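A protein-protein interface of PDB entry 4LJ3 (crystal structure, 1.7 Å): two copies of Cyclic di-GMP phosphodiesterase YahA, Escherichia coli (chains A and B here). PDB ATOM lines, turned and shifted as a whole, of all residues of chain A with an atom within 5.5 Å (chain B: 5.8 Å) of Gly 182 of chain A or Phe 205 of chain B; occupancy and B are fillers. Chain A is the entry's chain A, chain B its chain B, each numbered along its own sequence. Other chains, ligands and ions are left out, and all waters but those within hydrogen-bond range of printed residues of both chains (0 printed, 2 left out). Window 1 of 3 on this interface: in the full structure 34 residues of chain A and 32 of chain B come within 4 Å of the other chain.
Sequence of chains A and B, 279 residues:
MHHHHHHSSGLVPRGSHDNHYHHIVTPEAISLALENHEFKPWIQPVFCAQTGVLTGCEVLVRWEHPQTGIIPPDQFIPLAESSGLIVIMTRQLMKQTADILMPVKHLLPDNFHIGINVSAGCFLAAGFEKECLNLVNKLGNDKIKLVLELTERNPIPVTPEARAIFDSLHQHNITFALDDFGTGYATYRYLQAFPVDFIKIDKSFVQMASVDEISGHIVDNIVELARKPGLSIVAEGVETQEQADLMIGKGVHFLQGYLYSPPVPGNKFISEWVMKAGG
Glu 152 of chain A touches none of the printed residues of chain B.
Gly 182 of chain A touches just these residues of chain B: Phe 205 (3.9 Å), Met 208 (3.3 Å) and Ile 218 (3.8 Å).
Of the printed residues of chain B, Phe 205 of chain A touches Gly 182 (3.8 Å).
Of the printed residues of chain B, Ile 222 of chain A touches Ile 218 (3.5 Å).
Printed residues of chain A within 4 Å of Gly 182 of chain B: Phe 205.
Lys 203 of chain B touches none of the printed residues of chain A.
Phe 205 of chain B touches one residue of chain A.
Of the printed residues of chain A, Met 208 of chain B touches Gly 182 (3.3 Å), Thr 183 (3.9 Å) and Gly 184 (3.5 Å).
The nearest residue of chain A that does not touch Phe 205 of chain B is Phe 205 of chain A (4.2 Å).
Of the 10 printed residues of chain A, 5 touch a printed residue of chain B.
Printed residues of chain A that touch a printed residue of chain B: Gly 182, Thr 183, Gly 184, Phe 205 and Ile 222.
Hydrophobic or aromatic side chains of chain A within 4 Å of the printed part of chain B: Phe 205 and Ile 222.
Of the 16 printed residues of chain B, 4 touch a printed residue of chain A.
Printed residues of chain B that touch a printed residue of chain A: Gly 182, Phe 205, Met 208 and Ile 218.
Hydrophobic or aromatic side chains of chain B that line the printed part of chain A: Phe 205, Met 208 and Ile 218.
Among the printed residues, no Asp or Glu carboxylate lies within 4 Å of a Lys or Arg side-chain nitrogen of the other chain.
Among the printed residues, pairs that only touch across the chains: Gly 182 of chain A with Met 208 of chain B, Gly 184 of chain A with Met 208 of chain B, Ile 222 of chain A with Ile 218 of chain B, Phe 205 of chain A with Gly 182 of chain B, Gly 182 of chain A with Ile 218 of chain B, Thr 183 of chain A with Met 208 of chain B and Gly 182 of chain A with Phe 205 of chain B.
Gly 182 of chain A touches Phe 205 of chain B, and with the chains exchanged Phe 205 of chain A touches Gly 182 of chain B.
Positions printed for both chains: 180, 181, 182, 183, 202, 205 and 222.
The side-chain hydroxyl (OG1) of Thr 183 of chain A is in hydrogen-bond range of the backbone carbonyl oxygen (O) of Asp 180 of chain A, 2.7 Å away.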
ATOM      1  N   GLU A 152      16.650  -8.751  -3.015  1.00  0.00           N
ATOM      2  CA  GLU A 152      16.309  -9.063  -1.622  1.00  0.00           C
ATOM      3  C   GLU A 152      14.813  -9.297  -1.420  1.00  0.00           C
ATOM      4  O   GLU A 152      14.404  -9.840  -0.402  1.00  0.00           O
ATOM      5  CB  GLU A 152      16.750  -7.913  -0.732  1.00  0.00           C
ATOM      6  CG  GLU A 152      18.250  -7.745  -0.716  1.00  0.00           C
ATOM      7  CD  GLU A 152      18.656  -6.366  -0.242  1.00  0.00           C
ATOM      8  OE1 GLU A 152      18.978  -6.233   0.965  1.00  0.00           O
ATOM      9  OE2 GLU A 152      18.607  -5.435  -1.077  1.00  0.00           O
ATOM     10  N   ASP A 180      17.767  -3.087  -6.970  1.00  0.00           N
ATOM     11  CA  ASP A 180      16.961  -2.293  -6.027  1.00  0.00           C
ATOM     12  C   ASP A 180      17.667  -2.052  -4.672  1.00  0.00           C
ATOM     13  O   ASP A 180      17.078  -2.105  -3.565  1.00  0.00           O
ATOM     14  CB  ASP A 180      15.544  -2.893  -5.936  1.00  0.00           C
ATOM     15  CG  ASP A 180      14.878  -3.024  -7.357  1.00  0.00           C
ATOM     16  OD1 ASP A 180      15.218  -2.273  -8.309  1.00  0.00           O
ATOM     17  OD2 ASP A 180      13.996  -3.875  -7.536  1.00  0.00           O
ATOM     18  N   PHE A 181      18.954  -1.754  -4.789  1.00  0.00           N
ATOM     19  CA  PHE A 181      19.757  -1.426  -3.616  1.00  0.00           C
ATOM     20  C   PHE A 181      19.128  -0.233  -2.936  1.00  0.00           C
ATOM     21  O   PHE A 181      18.837   0.770  -3.599  1.00  0.00           O
ATOM     22  CB  PHE A 181      21.222  -1.138  -3.991  1.00  0.00           C
ATOM     23  CG  PHE A 181      22.125  -0.789  -2.795  1.00  0.00           C
ATOM     24  CD1 PHE A 181      22.786  -1.797  -2.093  1.00  0.00           C
ATOM     25  CD2 PHE A 181      22.309   0.520  -2.404  1.00  0.00           C
ATOM     26  CE1 PHE A 181      23.615  -1.515  -1.023  1.00  0.00           C
ATOM     27  CE2 PHE A 181      23.130   0.808  -1.319  1.00  0.00           C
ATOM     28  CZ  PHE A 181      23.777  -0.214  -0.636  1.00  0.00           C
ATOM     29  N   GLY A 182      18.951  -0.343  -1.622  1.00  0.00           N
ATOM     30  CA  GLY A 182      18.498   0.762  -0.795  1.00  0.00           C
ATOM     31  C   GLY A 182      17.106   0.510  -0.263  1.00  0.00           C
ATOM     32  O   GLY A 182      16.581   1.276   0.535  1.00  0.00           O
ATOM     33  N   THR A 183      16.530  -0.608  -0.695  1.00  0.00           N
ATOM     34  CA  THR A 183      15.171  -0.951  -0.357  1.00  0.00           C
ATOM     35  C   THR A 183      15.083  -2.263   0.450  1.00  0.00           C
ATOM     36  O   THR A 183      14.011  -2.576   0.933  1.00  0.00           O
ATOM     37  CB  THR A 183      14.302  -1.133  -1.615  1.00  0.00           C
ATOM     38  OG1 THR A 183      14.740  -2.290  -2.313  1.00  0.00           O
ATOM     39  CG2 THR A 183      14.366   0.070  -2.524  1.00  0.00           C
ATOM     40  N   GLY A 184      16.198  -2.987   0.629  1.00  0.00           N
ATOM     41  CA  GLY A 184      16.209  -4.280   1.298  1.00  0.00           C
ATOM     42  C   GLY A 184      16.302  -4.179   2.813  1.00  0.00           C
ATOM     43  O   GLY A 184      16.814  -3.182   3.340  1.00  0.00           O
ATOM     44  N   THR A 187      20.667  -5.635   4.108  1.00  0.00           N
ATOM     45  CA  THR A 187      21.461  -5.664   2.889  1.00  0.00           C
ATOM     46  C   THR A 187      22.909  -6.067   3.122  1.00  0.00           C
ATOM     47  O   THR A 187      23.474  -6.801   2.322  1.00  0.00           O
ATOM     48  CB  THR A 187      21.360  -4.310   2.142  1.00  0.00           C
ATOM     49  OG1 THR A 187      19.973  -4.030   1.927  1.00  0.00           O
ATOM     50  CG2 THR A 187      22.100  -4.333   0.804  1.00  0.00           C
ATOM     51  N   ASP A 202      18.401   1.506  -6.574  1.00  0.00           N
ATOM     52  CA  ASP A 202      16.977   1.549  -6.886  1.00  0.00           C
ATOM     53  C   ASP A 202      16.648   2.890  -7.536  1.00  0.00           C
ATOM     54  O   ASP A 202      17.196   3.923  -7.198  1.00  0.00           O
ATOM     55  CB  ASP A 202      16.109   1.353  -5.659  1.00  0.00           C
ATOM     56  CG  ASP A 202      14.613   1.119  -5.986  1.00  0.00           C
ATOM     57  OD1 ASP A 202      14.176  -0.053  -6.194  1.00  0.00           O
ATOM     58  OD2 ASP A 202      13.854   2.110  -5.975  1.00  0.00           O
ATOM     59  N   PHE A 205      15.872   6.270  -5.722  1.00  0.00           N
ATOM     60  CA  PHE A 205      16.987   7.101  -5.257  1.00  0.00           C
ATOM     61  C   PHE A 205      17.723   7.760  -6.404  1.00  0.00           C
ATOM     62  O   PHE A 205      18.144   8.925  -6.301  1.00  0.00           O
ATOM     63  CB  PHE A 205      17.964   6.302  -4.385  1.00  0.00           C
ATOM     64  CG  PHE A 205      17.287   5.519  -3.325  1.00  0.00           C
ATOM     65  CD1 PHE A 205      16.522   6.178  -2.364  1.00  0.00           C
ATOM     66  CD2 PHE A 205      17.304   4.144  -3.349  1.00  0.00           C
ATOM     67  CE1 PHE A 205      15.869   5.485  -1.386  1.00  0.00           C
ATOM     68  CE2 PHE A 205      16.650   3.429  -2.348  1.00  0.00           C
ATOM     69  CZ  PHE A 205      15.921   4.094  -1.387  1.00  0.00           C
ATOM     70  N   ILE A 222      22.451   6.658   0.344  1.00  0.00           N
ATOM     71  CA  ILE A 222      22.373   5.372  -0.355  1.00  0.00           C
ATOM     72  C   ILE A 222      23.614   5.126  -1.218  1.00  0.00           C
ATOM     73  O   ILE A 222      24.194   4.035  -1.166  1.00  0.00           O
ATOM     74  CB  ILE A 222      21.104   5.281  -1.247  1.00  0.00           C
ATOM     75  CG1 ILE A 222      19.806   5.320  -0.408  1.00  0.00           C
ATOM     76  CG2 ILE A 222      21.191   4.080  -2.172  1.00  0.00           C
ATOM     77  CD1 ILE A 222      19.705   4.281   0.666  1.00  0.00           C
ATOM     78  N   ASP B 180       4.503   7.318   2.185  1.00  0.00           N
ATOM     79  CA  ASP B 180       5.672   6.818   1.463  1.00  0.00           C
ATOM     80  C   ASP B 180       6.883   7.735   1.633  1.00  0.00           C
ATOM     81  O   ASP B 180       7.701   7.911   0.700  1.00  0.00           O
ATOM     82  CB  ASP B 180       5.367   6.736  -0.043  1.00  0.00           C
ATOM     83  CG  ASP B 180       4.150   5.853  -0.392  1.00  0.00           C
ATOM     84  OD1 ASP B 180       3.888   4.797   0.242  1.00  0.00           O
ATOM     85  OD2 ASP B 180       3.432   6.280  -1.345  1.00  0.00           O
ATOM     86  N   PHE B 181       7.028   8.316   2.823  1.00  0.00           N
ATOM     87  CA  PHE B 181       8.139   9.216   3.086  1.00  0.00           C
ATOM     88  C   PHE B 181       9.433   8.437   2.918  1.00  0.00           C
ATOM     89  O   PHE B 181       9.559   7.345   3.472  1.00  0.00           O
ATOM     90  CB  PHE B 181       8.048   9.832   4.497  1.00  0.00           C
ATOM     91  CG  PHE B 181       9.203  10.785   4.830  1.00  0.00           C
ATOM     92  CD1 PHE B 181       9.105  12.132   4.514  1.00  0.00           C
ATOM     93  CD2 PHE B 181      10.386  10.305   5.362  1.00  0.00           C
ATOM     94  CE1 PHE B 181      10.163  13.003   4.751  1.00  0.00           C
ATOM     95  CE2 PHE B 181      11.445  11.162   5.619  1.00  0.00           C
ATOM     96  CZ  PHE B 181      11.321  12.513   5.328  1.00  0.00           C
ATOM     97  N   GLY B 182      10.371   9.003   2.163  1.00  0.00           N
ATOM     98  CA  GLY B 182      11.690   8.426   1.977  1.00  0.00           C
ATOM     99  C   GLY B 182      11.870   7.889   0.566  1.00  0.00           C
ATOM    100  O   GLY B 182      12.967   7.465   0.162  1.00  0.00           O
ATOM    101  N   THR B 183      10.810   8.018  -0.223  1.00  0.00           N
ATOM    102  CA  THR B 183      10.811   7.511  -1.581  1.00  0.00           C
ATOM    103  C   THR B 183      10.639   8.625  -2.646  1.00  0.00           C
ATOM    104  O   THR B 183      10.793   8.335  -3.832  1.00  0.00           O
ATOM    105  CB  THR B 183       9.716   6.451  -1.773  1.00  0.00           C
ATOM    106  OG1 THR B 183       8.459   7.085  -1.698  1.00  0.00           O
ATOM    107  CG2 THR B 183       9.749   5.338  -0.733  1.00  0.00           C
ATOM    108  N   ILE B 201       6.343   7.139   7.408  1.00  0.00           N
ATOM    109  CA  ILE B 201       7.567   6.539   6.914  1.00  0.00           C
ATOM    110  C   ILE B 201       7.236   5.298   6.088  1.00  0.00           C
ATOM    111  O   ILE B 201       6.474   4.443   6.522  1.00  0.00           O
ATOM    112  CB  ILE B 201       8.544   6.263   8.057  1.00  0.00           C
ATOM    113  CG1 ILE B 201       8.947   7.652   8.592  1.00  0.00           C
ATOM    114  CG2 ILE B 201       9.767   5.507   7.514  1.00  0.00           C
ATOM    115  CD1 ILE B 201       9.564   7.663   9.938  1.00  0.00           C
ATOM    116  N   ASP B 202       7.780   5.207   4.885  1.00  0.00           N
ATOM    117  CA  ASP B 202       7.460   4.093   4.016  1.00  0.00           C
ATOM    118  C   ASP B 202       7.831   2.768   4.669  1.00  0.00           C
ATOM    119  O   ASP B 202       8.813   2.665   5.378  1.00  0.00           O
ATOM    120  CB  ASP B 202       8.163   4.186   2.683  1.00  0.00           C
ATOM    121  CG  ASP B 202       7.601   3.175   1.713  1.00  0.00           C
ATOM    122  OD1 ASP B 202       6.386   3.308   1.419  1.00  0.00           O
ATOM    123  OD2 ASP B 202       8.302   2.196   1.395  1.00  0.00           O
ATOM    124  N   LYS B 203       6.999   1.766   4.432  1.00  0.00           N
ATOM    125  CA  LYS B 203       7.160   0.455   5.022  1.00  0.00           C
ATOM    126  C   LYS B 203       8.520  -0.147   4.717  1.00  0.00           C
ATOM    127  O   LYS B 203       9.074  -0.857   5.540  1.00  0.00           O
ATOM    128  CB  LYS B 203       6.060  -0.501   4.560  1.00  0.00           C
ATOM    129  CG  LYS B 203       5.616  -0.339   3.127  1.00  0.00           C
ATOM    130  CD  LYS B 203       4.463  -1.264   2.838  1.00  0.00           C
ATOM    131  CE  LYS B 203       4.915  -2.532   2.158  1.00  0.00           C
ATOM    132  NZ  LYS B 203       3.748  -3.379   1.866  1.00  0.00           N
ATOM    133  N   SER B 204       9.047   0.095   3.527  1.00  0.00           N
ATOM    134  CA  SER B 204      10.383  -0.418   3.197  1.00  0.00           C
ATOM    135  C   SER B 204      11.420  -0.080   4.259  1.00  0.00           C
ATOM    136  O   SER B 204      12.258  -0.925   4.626  1.00  0.00           O
ATOM    137  CB  SER B 204      10.844   0.053   1.827  1.00  0.00           C
ATOM    138  OG  SER B 204      10.885   1.454   1.696  1.00  0.00           O
ATOM    139  N   PHE B 205      11.347   1.138   4.771  1.00  0.00           N
ATOM    140  CA  PHE B 205      12.337   1.571   5.790  1.00  0.00           C
ATOM    141  C   PHE B 205      11.965   1.102   7.185  1.00  0.00           C
ATOM    142  O   PHE B 205      12.829   0.735   7.979  1.00  0.00           O
ATOM    143  CB  PHE B 205      12.517   3.083   5.758  1.00  0.00           C
ATOM    144  CG  PHE B 205      12.788   3.607   4.408  1.00  0.00           C
ATOM    145  CD1 PHE B 205      13.939   3.226   3.738  1.00  0.00           C
ATOM    146  CD2 PHE B 205      11.866   4.411   3.768  1.00  0.00           C
ATOM    147  CE1 PHE B 205      14.220   3.697   2.473  1.00  0.00           C
ATOM    148  CE2 PHE B 205      12.146   4.906   2.491  1.00  0.00           C
ATOM    149  CZ  PHE B 205      13.294   4.519   1.834  1.00  0.00           C
ATOM    150  N   VAL B 206      10.682   1.086   7.495  1.00  0.00           N
ATOM    151  CA  VAL B 206      10.216   0.648   8.816  1.00  0.00           C
ATOM    152  C   VAL B 206      10.671  -0.792   9.080  1.00  0.00           C
ATOM    153  O   VAL B 206      10.953  -1.179  10.204  1.00  0.00           O
ATOM    154  CB  VAL B 206       8.665   0.765   8.912  1.00  0.00           C
ATOM    155  CG1 VAL B 206       8.140   0.072  10.153  1.00  0.00           C
ATOM    156  CG2 VAL B 206       8.234   2.213   8.857  1.00  0.00           C
ATOM    157  N   GLN B 207      10.751  -1.597   8.025  1.00  0.00           N
ATOM    158  CA  GLN B 207      11.088  -3.010   8.179  1.00  0.00           C
ATOM    159  C   GLN B 207      12.571  -3.290   8.128  1.00  0.00           C
ATOM    160  O   GLN B 207      12.963  -4.448   8.267  1.00  0.00           O
ATOM    161  CB  GLN B 207      10.382  -3.829   7.089  1.00  0.00           C
ATOM    162  CG  GLN B 207       8.882  -3.744   7.265  1.00  0.00           C
ATOM    163  CD  GLN B 207       8.110  -4.438   6.177  1.00  0.00           C
ATOM    164  OE1 GLN B 207       8.692  -4.944   5.199  1.00  0.00           O
ATOM    165  NE2 GLN B 207       6.803  -4.545   6.375  1.00  0.00           N
ATOM    166  N   MET B 208      13.404  -2.263   7.934  1.00  0.00           N
ATOM    167  CA  MET B 208      14.872  -2.463   7.975  1.00  0.00           C
ATOM    168  C   MET B 208      15.427  -2.819   9.363  1.00  0.00           C
ATOM    169  O   MET B 208      15.078  -2.200  10.348  1.00  0.00           O
ATOM    170  CB  MET B 208      15.599  -1.234   7.444  1.00  0.00           C
ATOM    171  CG  MET B 208      15.429  -1.109   5.938  1.00  0.00           C
ATOM    172  SD  MET B 208      16.133   0.362   5.204  1.00  0.00           S
ATOM    173  CE  MET B 208      15.631   0.094   3.483  1.00  0.00           C
ATOM    174  N   ILE B 218      20.343   3.232   6.701  1.00  0.00           N
ATOM    175  CA  ILE B 218      19.280   3.835   5.884  1.00  0.00           C
ATOM    176  C   ILE B 218      18.088   4.242   6.721  1.00  0.00           C
ATOM    177  O   ILE B 218      17.654   5.396   6.655  1.00  0.00           O
ATOM    178  CB  ILE B 218      18.812   2.887   4.739  1.00  0.00           C
ATOM    179  CG1 ILE B 218      20.011   2.497   3.863  1.00  0.00           C
ATOM    180  CG2 ILE B 218      17.665   3.540   3.966  1.00  0.00           C
ATOM    181  CD1 ILE B 218      19.740   1.490   2.769  1.00  0.00           C
ATOM    182  N   VAL B 219      17.516   3.320   7.501  1.00  0.00           N
ATOM    183  CA  VAL B 219      16.352   3.672   8.310  1.00  0.00           C
ATOM    184  C   VAL B 219      16.689   4.782   9.320  1.00  0.00           C
ATOM    185  O   VAL B 219      15.876   5.682   9.534  1.00  0.00           O
ATOM    186  CB  VAL B 219      15.662   2.449   8.977  1.00  0.00           C
ATOM    187  CG1 VAL B 219      16.587   1.729   9.938  1.00  0.00           C
ATOM    188  CG2 VAL B 219      14.380   2.876   9.673  1.00  0.00           C
ATOM    189  N   ILE B 222      16.536   8.003   7.301  1.00  0.00           N
ATOM    190  CA  ILE B 222      15.183   8.391   6.915  1.00  0.00           C
ATOM    191  C   ILE B 222      14.393   8.945   8.099  1.00  0.00           C
ATOM    192  O   ILE B 222      13.716   9.967   7.976  1.00  0.00           O
ATOM    193  CB  ILE B 222      14.377   7.207   6.299  1.00  0.00           C
ATOM    194  CG1 ILE B 222      14.987   6.736   4.961  1.00  0.00           C
ATOM    195  CG2 ILE B 222      12.918   7.543   6.197  1.00  0.00           C
ATOM    196  CD1 ILE B 222      15.136   7.796   3.902  1.00  0.00           C
ATOM    197  N   MET B 247      11.152   2.010  16.182  1.00  0.00           N
ATOM    198  CA  MET B 247      10.356   3.199  15.922  1.00  0.00           C
ATOM    199  C   MET B 247       9.949   3.932  17.208  1.00  0.00           C
ATOM    200  O   MET B 247      10.070   5.139  17.291  1.00  0.00           O
ATOM    201  CB  MET B 247       9.116   2.831  15.110  1.00  0.00           C
ATOM    202  CG  MET B 247       9.424   2.323  13.707  1.00  0.00           C
ATOM    203  SD  MET B 247      10.269   3.652  12.754  1.00  0.00           S
ATOM    204  CE  MET B 247      11.853   2.823  12.532  1.00  0.00           C
